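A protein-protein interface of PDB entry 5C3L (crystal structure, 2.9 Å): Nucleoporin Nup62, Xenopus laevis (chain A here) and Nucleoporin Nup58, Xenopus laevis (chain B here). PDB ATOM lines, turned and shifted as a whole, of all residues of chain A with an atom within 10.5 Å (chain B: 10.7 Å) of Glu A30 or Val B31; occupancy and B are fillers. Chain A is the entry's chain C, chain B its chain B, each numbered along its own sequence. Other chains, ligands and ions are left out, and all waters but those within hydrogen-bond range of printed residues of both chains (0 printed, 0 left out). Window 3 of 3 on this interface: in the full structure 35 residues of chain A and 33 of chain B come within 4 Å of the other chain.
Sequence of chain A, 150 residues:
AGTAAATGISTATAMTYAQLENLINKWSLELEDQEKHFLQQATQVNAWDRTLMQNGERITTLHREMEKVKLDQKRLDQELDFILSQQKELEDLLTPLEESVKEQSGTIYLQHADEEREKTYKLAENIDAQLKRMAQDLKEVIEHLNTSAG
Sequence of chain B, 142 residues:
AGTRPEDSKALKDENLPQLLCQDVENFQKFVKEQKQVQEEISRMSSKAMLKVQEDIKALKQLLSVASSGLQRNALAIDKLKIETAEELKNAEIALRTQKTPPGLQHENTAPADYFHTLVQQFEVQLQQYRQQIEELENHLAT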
ATOM      1  N   ASN A  22      40.364   5.621  18.724  1.00  0.00           N
ATOM      2  CA  ASN A  22      39.891   4.331  18.228  1.00  0.00           C
ATOM      3  C   ASN A  22      38.392   4.394  17.961  1.00  0.00           C
ATOM      4  O   ASN A  22      37.866   3.646  17.133  1.00  0.00           O
ATOM      5  CB  ASN A  22      40.206   3.207  19.220  1.00  0.00           C
ATOM      6  CG  ASN A  22      40.609   1.918  18.527  1.00  0.00           C
ATOM      7  OD1 ASN A  22      41.605   1.291  18.886  1.00  0.00           O
ATOM      8  ND2 ASN A  22      39.840   1.523  17.522  1.00  0.00           N
ATOM      9  N   LEU A  23      37.712   5.291  18.671  1.00  0.00           N
ATOM     10  CA  LEU A  23      36.294   5.531  18.446  1.00  0.00           C
ATOM     11  C   LEU A  23      36.086   6.004  17.015  1.00  0.00           C
ATOM     12  O   LEU A  23      35.204   5.512  16.320  1.00  0.00           O
ATOM     13  CB  LEU A  23      35.743   6.562  19.434  1.00  0.00           C
ATOM     14  CG  LEU A  23      35.996   6.270  20.914  1.00  0.00           C
ATOM     15  CD1 LEU A  23      37.003   7.258  21.486  1.00  0.00           C
ATOM     16  CD2 LEU A  23      34.693   6.304  21.692  1.00  0.00           C
ATOM     17  N   ILE A  24      36.920   6.941  16.573  1.00  0.00           N
ATOM     18  CA  ILE A  24      36.846   7.463  15.208  1.00  0.00           C
ATOM     19  C   ILE A  24      36.858   6.326  14.185  1.00  0.00           C
ATOM     20  O   ILE A  24      36.337   6.475  13.080  1.00  0.00           O
ATOM     21  CB  ILE A  24      38.001   8.454  14.929  1.00  0.00           C
ATOM     22  CG1 ILE A  24      37.636   9.827  15.500  1.00  0.00           C
ATOM     23  CG2 ILE A  24      38.303   8.561  13.429  1.00  0.00           C
ATOM     24  CD1 ILE A  24      38.776  10.805  15.534  1.00  0.00           C
ATOM     25  N   ASN A  25      37.428   5.185  14.565  1.00  0.00           N
ATOM     26  CA  ASN A  25      37.438   4.015  13.697  1.00  0.00           C
ATOM     27  C   ASN A  25      36.081   3.295  13.678  1.00  0.00           C
ATOM     28  O   ASN A  25      35.829   2.467  12.796  1.00  0.00           O
ATOM     29  CB  ASN A  25      38.541   3.046  14.133  1.00  0.00           C
ATOM     30  CG  ASN A  25      39.163   2.296  12.963  1.00  0.00           C
ATOM     31  OD1 ASN A  25      40.379   2.089  12.922  1.00  0.00           O
ATOM     32  ND2 ASN A  25      38.335   1.888  12.002  1.00  0.00           N
ATOM     33  N   LYS A  26      35.213   3.609  14.642  1.00  0.00           N
ATOM     34  CA  LYS A  26      33.849   3.072  14.657  1.00  0.00           C
ATOM     35  C   LYS A  26      32.954   3.897  13.743  1.00  0.00           C
ATOM     36  O   LYS A  26      32.407   3.374  12.777  1.00  0.00           O
ATOM     37  CB  LYS A  26      33.269   3.041  16.084  1.00  0.00           C
ATOM     38  CG  LYS A  26      31.758   3.313  16.190  1.00  0.00           C
ATOM     39  CD  LYS A  26      31.199   2.823  17.531  1.00  0.00           C
ATOM     40  CE  LYS A  26      30.024   3.670  18.034  1.00  0.00           C
ATOM     41  NZ  LYS A  26      28.822   3.636  17.150  1.00  0.00           N
ATOM     42  N   TRP A  27      32.826   5.186  14.044  1.00  0.00           N
ATOM     43  CA  TRP A  27      31.939   6.064  13.285  1.00  0.00           C
ATOM     44  C   TRP A  27      32.356   6.087  11.816  1.00  0.00           C
ATOM     45  O   TRP A  27      31.515   6.266  10.928  1.00  0.00           O
ATOM     46  CB  TRP A  27      31.932   7.503  13.831  1.00  0.00           C
ATOM     47  CG  TRP A  27      32.220   7.650  15.295  1.00  0.00           C
ATOM     48  CD1 TRP A  27      33.443   7.639  15.880  1.00  0.00           C
ATOM     49  CD2 TRP A  27      31.275   7.861  16.352  1.00  0.00           C
ATOM     50  NE1 TRP A  27      33.333   7.807  17.235  1.00  0.00           N
ATOM     51  CE2 TRP A  27      32.010   7.951  17.552  1.00  0.00           C
ATOM     52  CE3 TRP A  27      29.884   7.978  16.403  1.00  0.00           C
ATOM     53  CZ2 TRP A  27      31.403   8.150  18.786  1.00  0.00           C
ATOM     54  CZ3 TRP A  27      29.282   8.176  17.633  1.00  0.00           C
ATOM     55  CH2 TRP A  27      30.043   8.258  18.806  1.00  0.00           C
ATOM     56  N   SER A  28      33.650   5.905  11.561  1.00  0.00           N
ATOM     57  CA  SER A  28      34.157   5.906  10.191  1.00  0.00           C
ATOM     58  C   SER A  28      33.940   4.540   9.531  1.00  0.00           C
ATOM     59  O   SER A  28      34.191   4.368   8.339  1.00  0.00           O
ATOM     60  CB  SER A  28      35.640   6.295  10.165  1.00  0.00           C
ATOM     61  OG  SER A  28      36.092   6.561   8.846  1.00  0.00           O
ATOM     62  N   LEU A  29      33.459   3.573  10.304  1.00  0.00           N
ATOM     63  CA  LEU A  29      33.098   2.273   9.748  1.00  0.00           C
ATOM     64  C   LEU A  29      31.572   2.153   9.662  1.00  0.00           C
ATOM     65  O   LEU A  29      31.039   1.343   8.902  1.00  0.00           O
ATOM     66  CB  LEU A  29      33.697   1.145  10.588  1.00  0.00           C
ATOM     67  CG  LEU A  29      33.535  -0.260  10.003  1.00  0.00           C
ATOM     68  CD1 LEU A  29      34.025  -0.339   8.555  1.00  0.00           C
ATOM     69  CD2 LEU A  29      34.273  -1.259  10.870  1.00  0.00           C
ATOM     70  N   GLU A  30      30.881   2.973  10.450  1.00  0.00           N
ATOM     71  CA  GLU A  30      29.442   3.151  10.316  1.00  0.00           C
ATOM     72  C   GLU A  30      29.120   3.874   9.004  1.00  0.00           C
ATOM     73  O   GLU A  30      28.233   3.461   8.261  1.00  0.00           O
ATOM     74  CB  GLU A  30      28.886   3.943  11.500  1.00  0.00           C
ATOM     75  CG  GLU A  30      28.960   3.224  12.835  1.00  0.00           C
ATOM     76  CD  GLU A  30      28.294   4.008  13.961  1.00  0.00           C
ATOM     77  OE1 GLU A  30      28.002   5.210  13.764  1.00  0.00           O
ATOM     78  OE2 GLU A  30      28.056   3.420  15.041  1.00  0.00           O
ATOM     79  N   LEU A  31      29.841   4.962   8.732  1.00  0.00           N
ATOM     80  CA  LEU A  31      29.709   5.684   7.467  1.00  0.00           C
ATOM     81  C   LEU A  31      30.101   4.787   6.295  1.00  0.00           C
ATOM     82  O   LEU A  31      29.671   5.008   5.163  1.00  0.00           O
ATOM     83  CB  LEU A  31      30.565   6.957   7.474  1.00  0.00           C
ATOM     84  CG  LEU A  31      29.801   8.249   7.792  1.00  0.00           C
ATOM     85  CD1 LEU A  31      29.087   8.156   9.139  1.00  0.00           C
ATOM     86  CD2 LEU A  31      30.728   9.458   7.749  1.00  0.00           C
ATOM     87  N   GLU A  32      30.919   3.778   6.577  1.00  0.00           N
ATOM     88  CA  GLU A  32      31.185   2.709   5.622  1.00  0.00           C
ATOM     89  C   GLU A  32      30.173   1.577   5.852  1.00  0.00           C
ATOM     90  O   GLU A  32      30.467   0.398   5.641  1.00  0.00           O
ATOM     91  CB  GLU A  32      32.628   2.204   5.762  1.00  0.00           C
ATOM     92  CG  GLU A  32      33.068   1.265   4.646  1.00  0.00           C
ATOM     93  CD  GLU A  32      34.150   1.855   3.765  1.00  0.00           C
ATOM     94  OE1 GLU A  32      35.217   2.242   4.296  1.00  0.00           O
ATOM     95  OE2 GLU A  32      33.927   1.928   2.535  1.00  0.00           O
ATOM     96  N   ASP A  33      28.979   1.960   6.306  1.00  0.00           N
ATOM     97  CA  ASP A  33      27.836   1.053   6.442  1.00  0.00           C
ATOM     98  C   ASP A  33      26.520   1.815   6.160  1.00  0.00           C
ATOM     99  O   ASP A  33      25.490   1.202   5.879  1.00  0.00           O
ATOM    100  CB  ASP A  33      27.837   0.404   7.843  1.00  0.00           C
ATOM    101  CG  ASP A  33      26.444   0.240   8.431  1.00  0.00           C
ATOM    102  OD1 ASP A  33      25.794  -0.793   8.156  1.00  0.00           O
ATOM    103  OD2 ASP A  33      26.002   1.137   9.183  1.00  0.00           O
ATOM    104  N   GLN A  34      26.575   3.146   6.200  1.00  0.00           N
ATOM    105  CA  GLN A  34      25.410   4.003   5.962  1.00  0.00           C
ATOM    106  C   GLN A  34      25.442   4.634   4.568  1.00  0.00           C
ATOM    107  O   GLN A  34      24.413   5.074   4.046  1.00  0.00           O
ATOM    108  CB  GLN A  34      25.336   5.109   7.018  1.00  0.00           C
ATOM    109  CG  GLN A  34      25.059   4.609   8.413  1.00  0.00           C
ATOM    110  CD  GLN A  34      23.584   4.505   8.715  1.00  0.00           C
ATOM    111  OE1 GLN A  34      22.937   5.499   9.057  1.00  0.00           O
ATOM    112  NE2 GLN A  34      23.041   3.296   8.608  1.00  0.00           N
ATOM    113  N   GLU A  35      26.625   4.700   3.971  1.00  0.00           N
ATOM    114  CA  GLU A  35      26.742   5.247   2.632  1.00  0.00           C
ATOM    115  C   GLU A  35      26.001   4.354   1.650  1.00  0.00           C
ATOM    116  O   GLU A  35      25.149   4.821   0.901  1.00  0.00           O
ATOM    117  CB  GLU A  35      28.203   5.383   2.218  1.00  0.00           C
ATOM    118  CG  GLU A  35      28.381   5.877   0.795  1.00  0.00           C
ATOM    119  CD  GLU A  35      29.830   5.886   0.356  1.00  0.00           C
ATOM    120  OE1 GLU A  35      30.699   5.520   1.177  1.00  0.00           O
ATOM    121  OE2 GLU A  35      30.102   6.249  -0.809  1.00  0.00           O
ATOM    122  N   LYS A  36      26.330   3.068   1.655  1.00  0.00           N
ATOM    123  CA  LYS A  36      25.708   2.127   0.730  1.00  0.00           C
ATOM    124  C   LYS A  36      24.201   2.010   0.984  1.00  0.00           C
ATOM    125  O   LYS A  36      23.449   1.648   0.077  1.00  0.00           O
ATOM    126  CB  LYS A  36      26.386   0.748   0.812  1.00  0.00           C
ATOM    127  CG  LYS A  36      26.129  -0.069   2.085  1.00  0.00           C
ATOM    128  CD  LYS A  36      26.848   0.475   3.318  1.00  0.00           C
ATOM    129  CE  LYS A  36      28.375   0.550   3.156  1.00  0.00           C
ATOM    130  NZ  LYS A  36      28.911   1.944   3.285  1.00  0.00           N
ATOM    131  N   HIS A  37      23.756   2.333   2.196  1.00  0.00           N
ATOM    132  CA  HIS A  37      22.324   2.398   2.464  1.00  0.00           C
ATOM    133  C   HIS A  37      21.754   3.579   1.699  1.00  0.00           C
ATOM    134  O   HIS A  37      20.763   3.447   0.977  1.00  0.00           O
ATOM    135  CB  HIS A  37      22.026   2.537   3.960  1.00  0.00           C
ATOM    136  CG  HIS A  37      21.967   1.234   4.696  1.00  0.00           C
ATOM    137  ND1 HIS A  37      21.308   1.084   5.892  1.00  0.00           N
ATOM    138  CD2 HIS A  37      22.495   0.018   4.398  1.00  0.00           C
ATOM    139  CE1 HIS A  37      21.425  -0.170   6.307  1.00  0.00           C
ATOM    140  NE2 HIS A  37      22.142  -0.831   5.418  1.00  0.00           N
ATOM    141  N   PHE A  38      22.400   4.733   1.852  1.00  0.00           N
ATOM    142  CA  PHE A  38      21.953   5.962   1.197  1.00  0.00           C
ATOM    143  C   PHE A  38      21.779   5.771  -0.309  1.00  0.00           C
ATOM    144  O   PHE A  38      20.745   6.134  -0.870  1.00  0.00           O
ATOM    145  CB  PHE A  38      22.939   7.103   1.455  1.00  0.00           C
ATOM    146  CG  PHE A  38      22.495   8.421   0.891  1.00  0.00           C
ATOM    147  CD1 PHE A  38      21.654   9.253   1.613  1.00  0.00           C
ATOM    148  CD2 PHE A  38      22.910   8.828  -0.363  1.00  0.00           C
ATOM    149  CE1 PHE A  38      21.244  10.469   1.092  1.00  0.00           C
ATOM    150  CE2 PHE A  38      22.497  10.028  -0.882  1.00  0.00           C
ATOM    151  CZ  PHE A  38      21.664  10.854  -0.151  1.00  0.00           C
ATOM    152  N   ASP B  23      32.769  18.504  20.671  1.00  0.00           N
ATOM    153  CA  ASP B  23      32.267  18.430  19.300  1.00  0.00           C
ATOM    154  C   ASP B  23      32.152  16.976  18.842  1.00  0.00           C
ATOM    155  O   ASP B  23      31.802  16.707  17.694  1.00  0.00           O
ATOM    156  CB  ASP B  23      33.177  19.205  18.343  1.00  0.00           C
ATOM    157  CG  ASP B  23      33.076  20.708  18.521  1.00  0.00           C
ATOM    158  OD1 ASP B  23      32.478  21.156  19.522  1.00  0.00           O
ATOM    159  OD2 ASP B  23      33.605  21.443  17.660  1.00  0.00           O
ATOM    160  N   VAL B  24      32.484  16.047  19.734  1.00  0.00           N
ATOM    161  CA  VAL B  24      32.144  14.643  19.543  1.00  0.00           C
ATOM    162  C   VAL B  24      30.650  14.462  19.807  1.00  0.00           C
ATOM    163  O   VAL B  24      30.014  13.574  19.239  1.00  0.00           O
ATOM    164  CB  VAL B  24      32.962  13.724  20.473  1.00  0.00           C
ATOM    165  CG1 VAL B  24      32.532  12.267  20.310  1.00  0.00           C
ATOM    166  CG2 VAL B  24      34.450  13.883  20.196  1.00  0.00           C
ATOM    167  N   GLU B  25      30.099  15.306  20.677  1.00  0.00           N
ATOM    168  CA  GLU B  25      28.656  15.346  20.893  1.00  0.00           C
ATOM    169  C   GLU B  25      27.998  16.026  19.693  1.00  0.00           C
ATOM    170  O   GLU B  25      26.819  15.805  19.408  1.00  0.00           O
ATOM    171  CB  GLU B  25      28.314  16.071  22.206  1.00  0.00           C
ATOM    172  CG  GLU B  25      27.594  17.408  22.049  1.00  0.00           C
ATOM    173  CD  GLU B  25      27.179  18.015  23.379  1.00  0.00           C
ATOM    174  OE1 GLU B  25      27.464  17.407  24.433  1.00  0.00           O
ATOM    175  OE2 GLU B  25      26.562  19.102  23.369  1.00  0.00           O
ATOM    176  N   ASN B  26      28.778  16.850  18.994  1.00  0.00           N
ATOM    177  CA  ASN B  26      28.363  17.442  17.724  1.00  0.00           C
ATOM    178  C   ASN B  26      28.536  16.451  16.568  1.00  0.00           C
ATOM    179  O   ASN B  26      28.414  16.818  15.400  1.00  0.00           O
ATOM    180  CB  ASN B  26      29.164  18.721  17.434  1.00  0.00           C
ATOM    181  CG  ASN B  26      29.028  19.767  18.530  1.00  0.00           C
ATOM    182  OD1 ASN B  26      28.578  19.470  19.636  1.00  0.00           O
ATOM    183  ND2 ASN B  26      29.430  21.000  18.225  1.00  0.00           N
ATOM    184  N   PHE B  27      28.839  15.201  16.910  1.00  0.00           N
ATOM    185  CA  PHE B  27      29.014  14.130  15.933  1.00  0.00           C
ATOM    186  C   PHE B  27      28.398  12.840  16.476  1.00  0.00           C
ATOM    187  O   PHE B  27      28.624  11.754  15.945  1.00  0.00           O
ATOM    188  CB  PHE B  27      30.498  13.934  15.617  1.00  0.00           C
ATOM    189  CG  PHE B  27      30.763  13.031  14.445  1.00  0.00           C
ATOM    190  CD1 PHE B  27      30.556  13.473  13.153  1.00  0.00           C
ATOM    191  CD2 PHE B  27      31.242  11.745  14.636  1.00  0.00           C
ATOM    192  CE1 PHE B  27      30.807  12.647  12.074  1.00  0.00           C
ATOM    193  CE2 PHE B  27      31.493  10.915  13.562  1.00  0.00           C
ATOM    194  CZ  PHE B  27      31.278  11.368  12.281  1.00  0.00           C
ATOM    195  N   GLN B  28      27.619  12.973  17.545  1.00  0.00           N
ATOM    196  CA  GLN B  28      26.928  11.843  18.149  1.00  0.00           C
ATOM    197  C   GLN B  28      25.439  11.970  17.885  1.00  0.00           C
ATOM    198  O   GLN B  28      24.800  11.041  17.390  1.00  0.00           O
ATOM    199  CB  GLN B  28      27.193  11.779  19.656  1.00  0.00           C
ATOM    200  CG  GLN B  28      27.929  10.531  20.110  1.00  0.00           C
ATOM    201  CD  GLN B  28      27.116   9.257  19.921  1.00  0.00           C
ATOM    202  OE1 GLN B  28      26.128   9.236  19.187  1.00  0.00           O
ATOM    203  NE2 GLN B  28      27.530   8.187  20.591  1.00  0.00           N
ATOM    204  N   LYS B  29      24.897  13.134  18.217  1.00  0.00           N
ATOM    205  CA  LYS B  29      23.478  13.392  18.040  1.00  0.00           C
ATOM    206  C   LYS B  29      23.091  13.335  16.565  1.00  0.00           C
ATOM    207  O   LYS B  29      21.991  12.903  16.219  1.00  0.00           O
ATOM    208  CB  LYS B  29      23.114  14.750  18.636  1.00  0.00           C
ATOM    209  CG  LYS B  29      23.274  14.803  20.145  1.00  0.00           C
ATOM    210  CD  LYS B  29      22.806  16.131  20.711  1.00  0.00           C
ATOM    211  CE  LYS B  29      22.666  16.061  22.222  1.00  0.00           C
ATOM    212  NZ  LYS B  29      22.092  17.312  22.787  1.00  0.00           N
ATOM    213  N   PHE B  30      24.011  13.749  15.701  1.00  0.00           N
ATOM    214  CA  PHE B  30      23.749  13.798  14.267  1.00  0.00           C
ATOM    215  C   PHE B  30      23.709  12.402  13.661  1.00  0.00           C
ATOM    216  O   PHE B  30      22.848  12.103  12.837  1.00  0.00           O
ATOM    217  CB  PHE B  30      24.810  14.640  13.558  1.00  0.00           C
ATOM    218  CG  PHE B  30      24.832  16.076  13.990  1.00  0.00           C
ATOM    219  CD1 PHE B  30      25.387  16.438  15.210  1.00  0.00           C
ATOM    220  CD2 PHE B  30      24.306  17.068  13.176  1.00  0.00           C
ATOM    221  CE1 PHE B  30      25.412  17.761  15.613  1.00  0.00           C
ATOM    222  CE2 PHE B  30      24.327  18.396  13.573  1.00  0.00           C
ATOM    223  CZ  PHE B  30      24.882  18.743  14.794  1.00  0.00           C
ATOM    224  N   VAL B  31      24.645  11.550  14.065  1.00  0.00           N
ATOM    225  CA  VAL B  31      24.719  10.196  13.534  1.00  0.00           C
ATOM    226  C   VAL B  31      23.413   9.449  13.774  1.00  0.00           C
ATOM    227  O   VAL B  31      22.972   8.675  12.925  1.00  0.00           O
ATOM    228  CB  VAL B  31      25.879   9.404  14.167  1.00  0.00           C
ATOM    229  CG1 VAL B  31      25.876   7.951  13.683  1.00  0.00           C
ATOM    230  CG2 VAL B  31      27.205  10.074  13.855  1.00  0.00           C
ATOM    231  N   LYS B  32      22.800   9.682  14.931  1.00  0.00           N
ATOM    232  CA  LYS B  32      21.535   9.037  15.270  1.00  0.00           C
ATOM    233  C   LYS B  32      20.396   9.576  14.422  1.00  0.00           C
ATOM    234  O   LYS B  32      19.620   8.803  13.862  1.00  0.00           O
ATOM    235  CB  LYS B  32      21.206   9.237  16.743  1.00  0.00           C
ATOM    236  CG  LYS B  32      22.273   8.742  17.691  1.00  0.00           C
ATOM    237  CD  LYS B  32      21.693   8.454  19.063  1.00  0.00           C
ATOM    238  CE  LYS B  32      20.787   9.582  19.545  1.00  0.00           C
ATOM    239  NZ  LYS B  32      21.430  10.922  19.448  1.00  0.00           N
ATOM    240  N   GLU B  33      20.299  10.903  14.349  1.00  0.00           N
ATOM    241  CA  GLU B  33      19.329  11.571  13.485  1.00  0.00           C
ATOM    242  C   GLU B  33      19.338  10.926  12.103  1.00  0.00           C
ATOM    243  O   GLU B  33      18.291  10.571  11.568  1.00  0.00           O
ATOM    244  CB  GLU B  33      19.641  13.068  13.377  1.00  0.00           C
ATOM    245  CG  GLU B  33      19.406  13.870  14.661  1.00  0.00           C
ATOM    246  CD  GLU B  33      18.015  14.488  14.743  1.00  0.00           C
ATOM    247  OE1 GLU B  33      17.840  15.448  15.527  1.00  0.00           O
ATOM    248  OE2 GLU B  33      17.101  14.021  14.031  1.00  0.00           O
ATOM    249  N   GLN B  34      20.534  10.742  11.553  1.00  0.00           N
ATOM    250  CA  GLN B  34      20.697  10.127  10.238  1.00  0.00           C
ATOM    251  C   GLN B  34      20.429   8.628  10.296  1.00  0.00           C
ATOM    252  O   GLN B  34      20.166   7.995   9.271  1.00  0.00           O
ATOM    253  CB  GLN B  34      22.108  10.391   9.691  1.00  0.00           C
ATOM    254  CG  GLN B  34      22.197  11.574   8.725  1.00  0.00           C
ATOM    255  CD  GLN B  34      21.593  12.833   9.304  1.00  0.00           C
ATOM    256  OE1 GLN B  34      21.475  12.971  10.518  1.00  0.00           O
ATOM    257  NE2 GLN B  34      21.193  13.754   8.438  1.00  0.00           N
ATOM    258  N   LYS B  35      20.489   8.064  11.495  1.00  0.00           N
ATOM    259  CA  LYS B  35      20.250   6.640  11.672  1.00  0.00           C
ATOM    260  C   LYS B  35      18.766   6.373  11.886  1.00  0.00           C
ATOM    261  O   LYS B  35      18.233   5.383  11.393  1.00  0.00           O
ATOM    262  CB  LYS B  35      21.059   6.096  12.853  1.00  0.00           C
ATOM    263  CG  LYS B  35      21.283   4.594  12.810  1.00  0.00           C
ATOM    264  CD  LYS B  35      22.163   4.210  11.633  1.00  0.00           C
ATOM    265  CE  LYS B  35      22.540   2.745  11.675  1.00  0.00           C
ATOM    266  NZ  LYS B  35      21.371   1.859  11.426  1.00  0.00           N
ATOM    267  N   GLN B  36      18.100   7.263  12.614  1.00  0.00           N
ATOM    268  CA  GLN B  36      16.697   7.059  12.951  1.00  0.00           C
ATOM    269  C   GLN B  36      15.783   7.446  11.781  1.00  0.00           C
ATOM    270  O   GLN B  36      14.640   6.997  11.713  1.00  0.00           O
ATOM    271  CB  GLN B  36      16.332   7.835  14.225  1.00  0.00           C
ATOM    272  CG  GLN B  36      16.506   9.343  14.154  1.00  0.00           C
ATOM    273  CD  GLN B  36      16.513   9.993  15.533  1.00  0.00           C
ATOM    274  OE1 GLN B  36      16.462   9.310  16.555  1.00  0.00           O
ATOM    275  NE2 GLN B  36      16.573  11.320  15.563  1.00  0.00           N
ATOM    276  N   VAL B  37      16.287   8.257  10.856  1.00  0.00           N
ATOM    277  CA  VAL B  37      15.573   8.498   9.605  1.00  0.00           C
ATOM    278  C   VAL B  37      15.789   7.308   8.684  1.00  0.00           C
ATOM    279  O   VAL B  37      14.854   6.841   8.044  1.00  0.00           O
ATOM    280  CB  VAL B  37      16.025   9.799   8.882  1.00  0.00           C
ATOM    281  CG1 VAL B  37      15.635  11.031   9.696  1.00  0.00           C
ATOM    282  CG2 VAL B  37      17.520   9.776   8.571  1.00  0.00           C
ATOM    283  N   GLN B  38      17.020   6.807   8.628  1.00  0.00           N
ATOM    284  CA  GLN B  38      17.329   5.667   7.776  1.00  0.00           C
ATOM    285  C   GLN B  38      16.416   4.509   8.123  1.00  0.00           C
ATOM    286  O   GLN B  38      16.085   3.690   7.269  1.00  0.00           O
ATOM    287  CB  GLN B  38      18.787   5.238   7.923  1.00  0.00           C
ATOM    288  CG  GLN B  38      19.165   4.063   7.030  1.00  0.00           C
ATOM    289  CD  GLN B  38      19.428   2.786   7.806  1.00  0.00           C
ATOM    290  OE1 GLN B  38      20.558   2.311   7.861  1.00  0.00           O
ATOM    291  NE2 GLN B  38      18.384   2.215   8.396  1.00  0.00           N
ATOM    292  N   GLU B  39      16.022   4.440   9.389  1.00  0.00           N
ATOM    293  CA  GLU B  39      15.092   3.417   9.832  1.00  0.00           C
ATOM    294  C   GLU B  39      13.685   3.759   9.359  1.00  0.00           C
ATOM    295  O   GLU B  39      12.914   2.867   9.009  1.00  0.00           O
ATOM    296  CB  GLU B  39      15.133   3.268  11.356  1.00  0.00           C
ATOM    297  CG  GLU B  39      16.434   2.662  11.883  1.00  0.00           C
ATOM    298  CD  GLU B  39      16.661   1.242  11.392  1.00  0.00           C
ATOM    299  OE1 GLU B  39      15.685   0.603  10.943  1.00  0.00           O
ATOM    300  OE2 GLU B  39      17.813   0.761  11.451  1.00  0.00           O
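The side-chain amide oxygen of Gln B38 is in hydrogen-bond range of the side-chain amide nitrogen of Gln A34.
OE1 of Gln B38 lies within hydrogen-bond range of ND1 of His A37 (2.4 Å).
The indole nitrogen of Trp A27 sits close to the backbone carbonyl oxygen of Leu A23 (3.1 Å).
The side-chain amino group (NZ) of Lys A26 lies within salt-bridge range of the side-chain carboxylate (OE1) of Glu A30 (3.8 Å).
O of Phe B30 sits close to OE1 of Gln B34 (2.8 Å).
NE2 of Gln B38 is in hydrogen-bond range of OE2 of Glu B39 (3.4 Å).
OE2 of Glu B39 lies within salt-bridge range of NZ of Lys B35, 3.7 Å away.
Trp A27 touches Phe B27.
Gln B28 touches Trp A27.
OE1 of Glu A30 touches CG1 of Val B31, 3.5 Å away.
OE1 of Gln A34 touches O of Gln B34 (3.7 Å).
Lys B35 touches Gln A34 (CD to OE1, 3.0 Å).
No residue of chain B comes within 4 Å of Lys A26.
Of the printed residues of chain B, Trp A27 touches Phe B27 and Gln B28.
Ser A28 touches none of the printed residues of chain B.
Glu A30 touches one residue of chain B.
No residue of chain B comes within 4 Å of Asp A33.
Of the printed residues of chain B, Gln A34 touches Gln B34, Lys B35 and Gln B38.
Phe B27 touches just one residue of chain A: Trp A27.
Of the printed residues of chain A, Gln B28 touches Trp A27.
Val B31 touches just one residue of chain A: Glu A30 (3.5 Å).
Lys B32 touches none of the printed residues of chain A.
Of the printed residues of chain A, Gln B34 touches Gln A34 (3.7 Å).
Printed residues of chain A within 4 Å of Lys B35: Gln A34.
Of the printed residues of chain A, Gln B38 touches Gln A34 and His A37.
The nearest residue of chain A that does not touch Val B31 is Trp A27 (4.3 Å).
The nearest printed residue of chain A that does not touch Gln B38 is Asp A33 (5.4 Å).
Hydrophobic or aromatic side chains of chain B that line the printed part of chain A: Phe B27 and Val B31.
Of the 17 printed residues of chain A, 4 touch a printed residue of chain B.
Printed residues of chain A that touch a printed residue of chain B: Trp A27, Glu A30, Gln A34 and His A37.
Hydrophobic or aromatic side chains of chain A within 4 Å of the printed part of chain B: Trp A27 and His A37.
Among the printed residues, 7 pairs touch across the chains.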
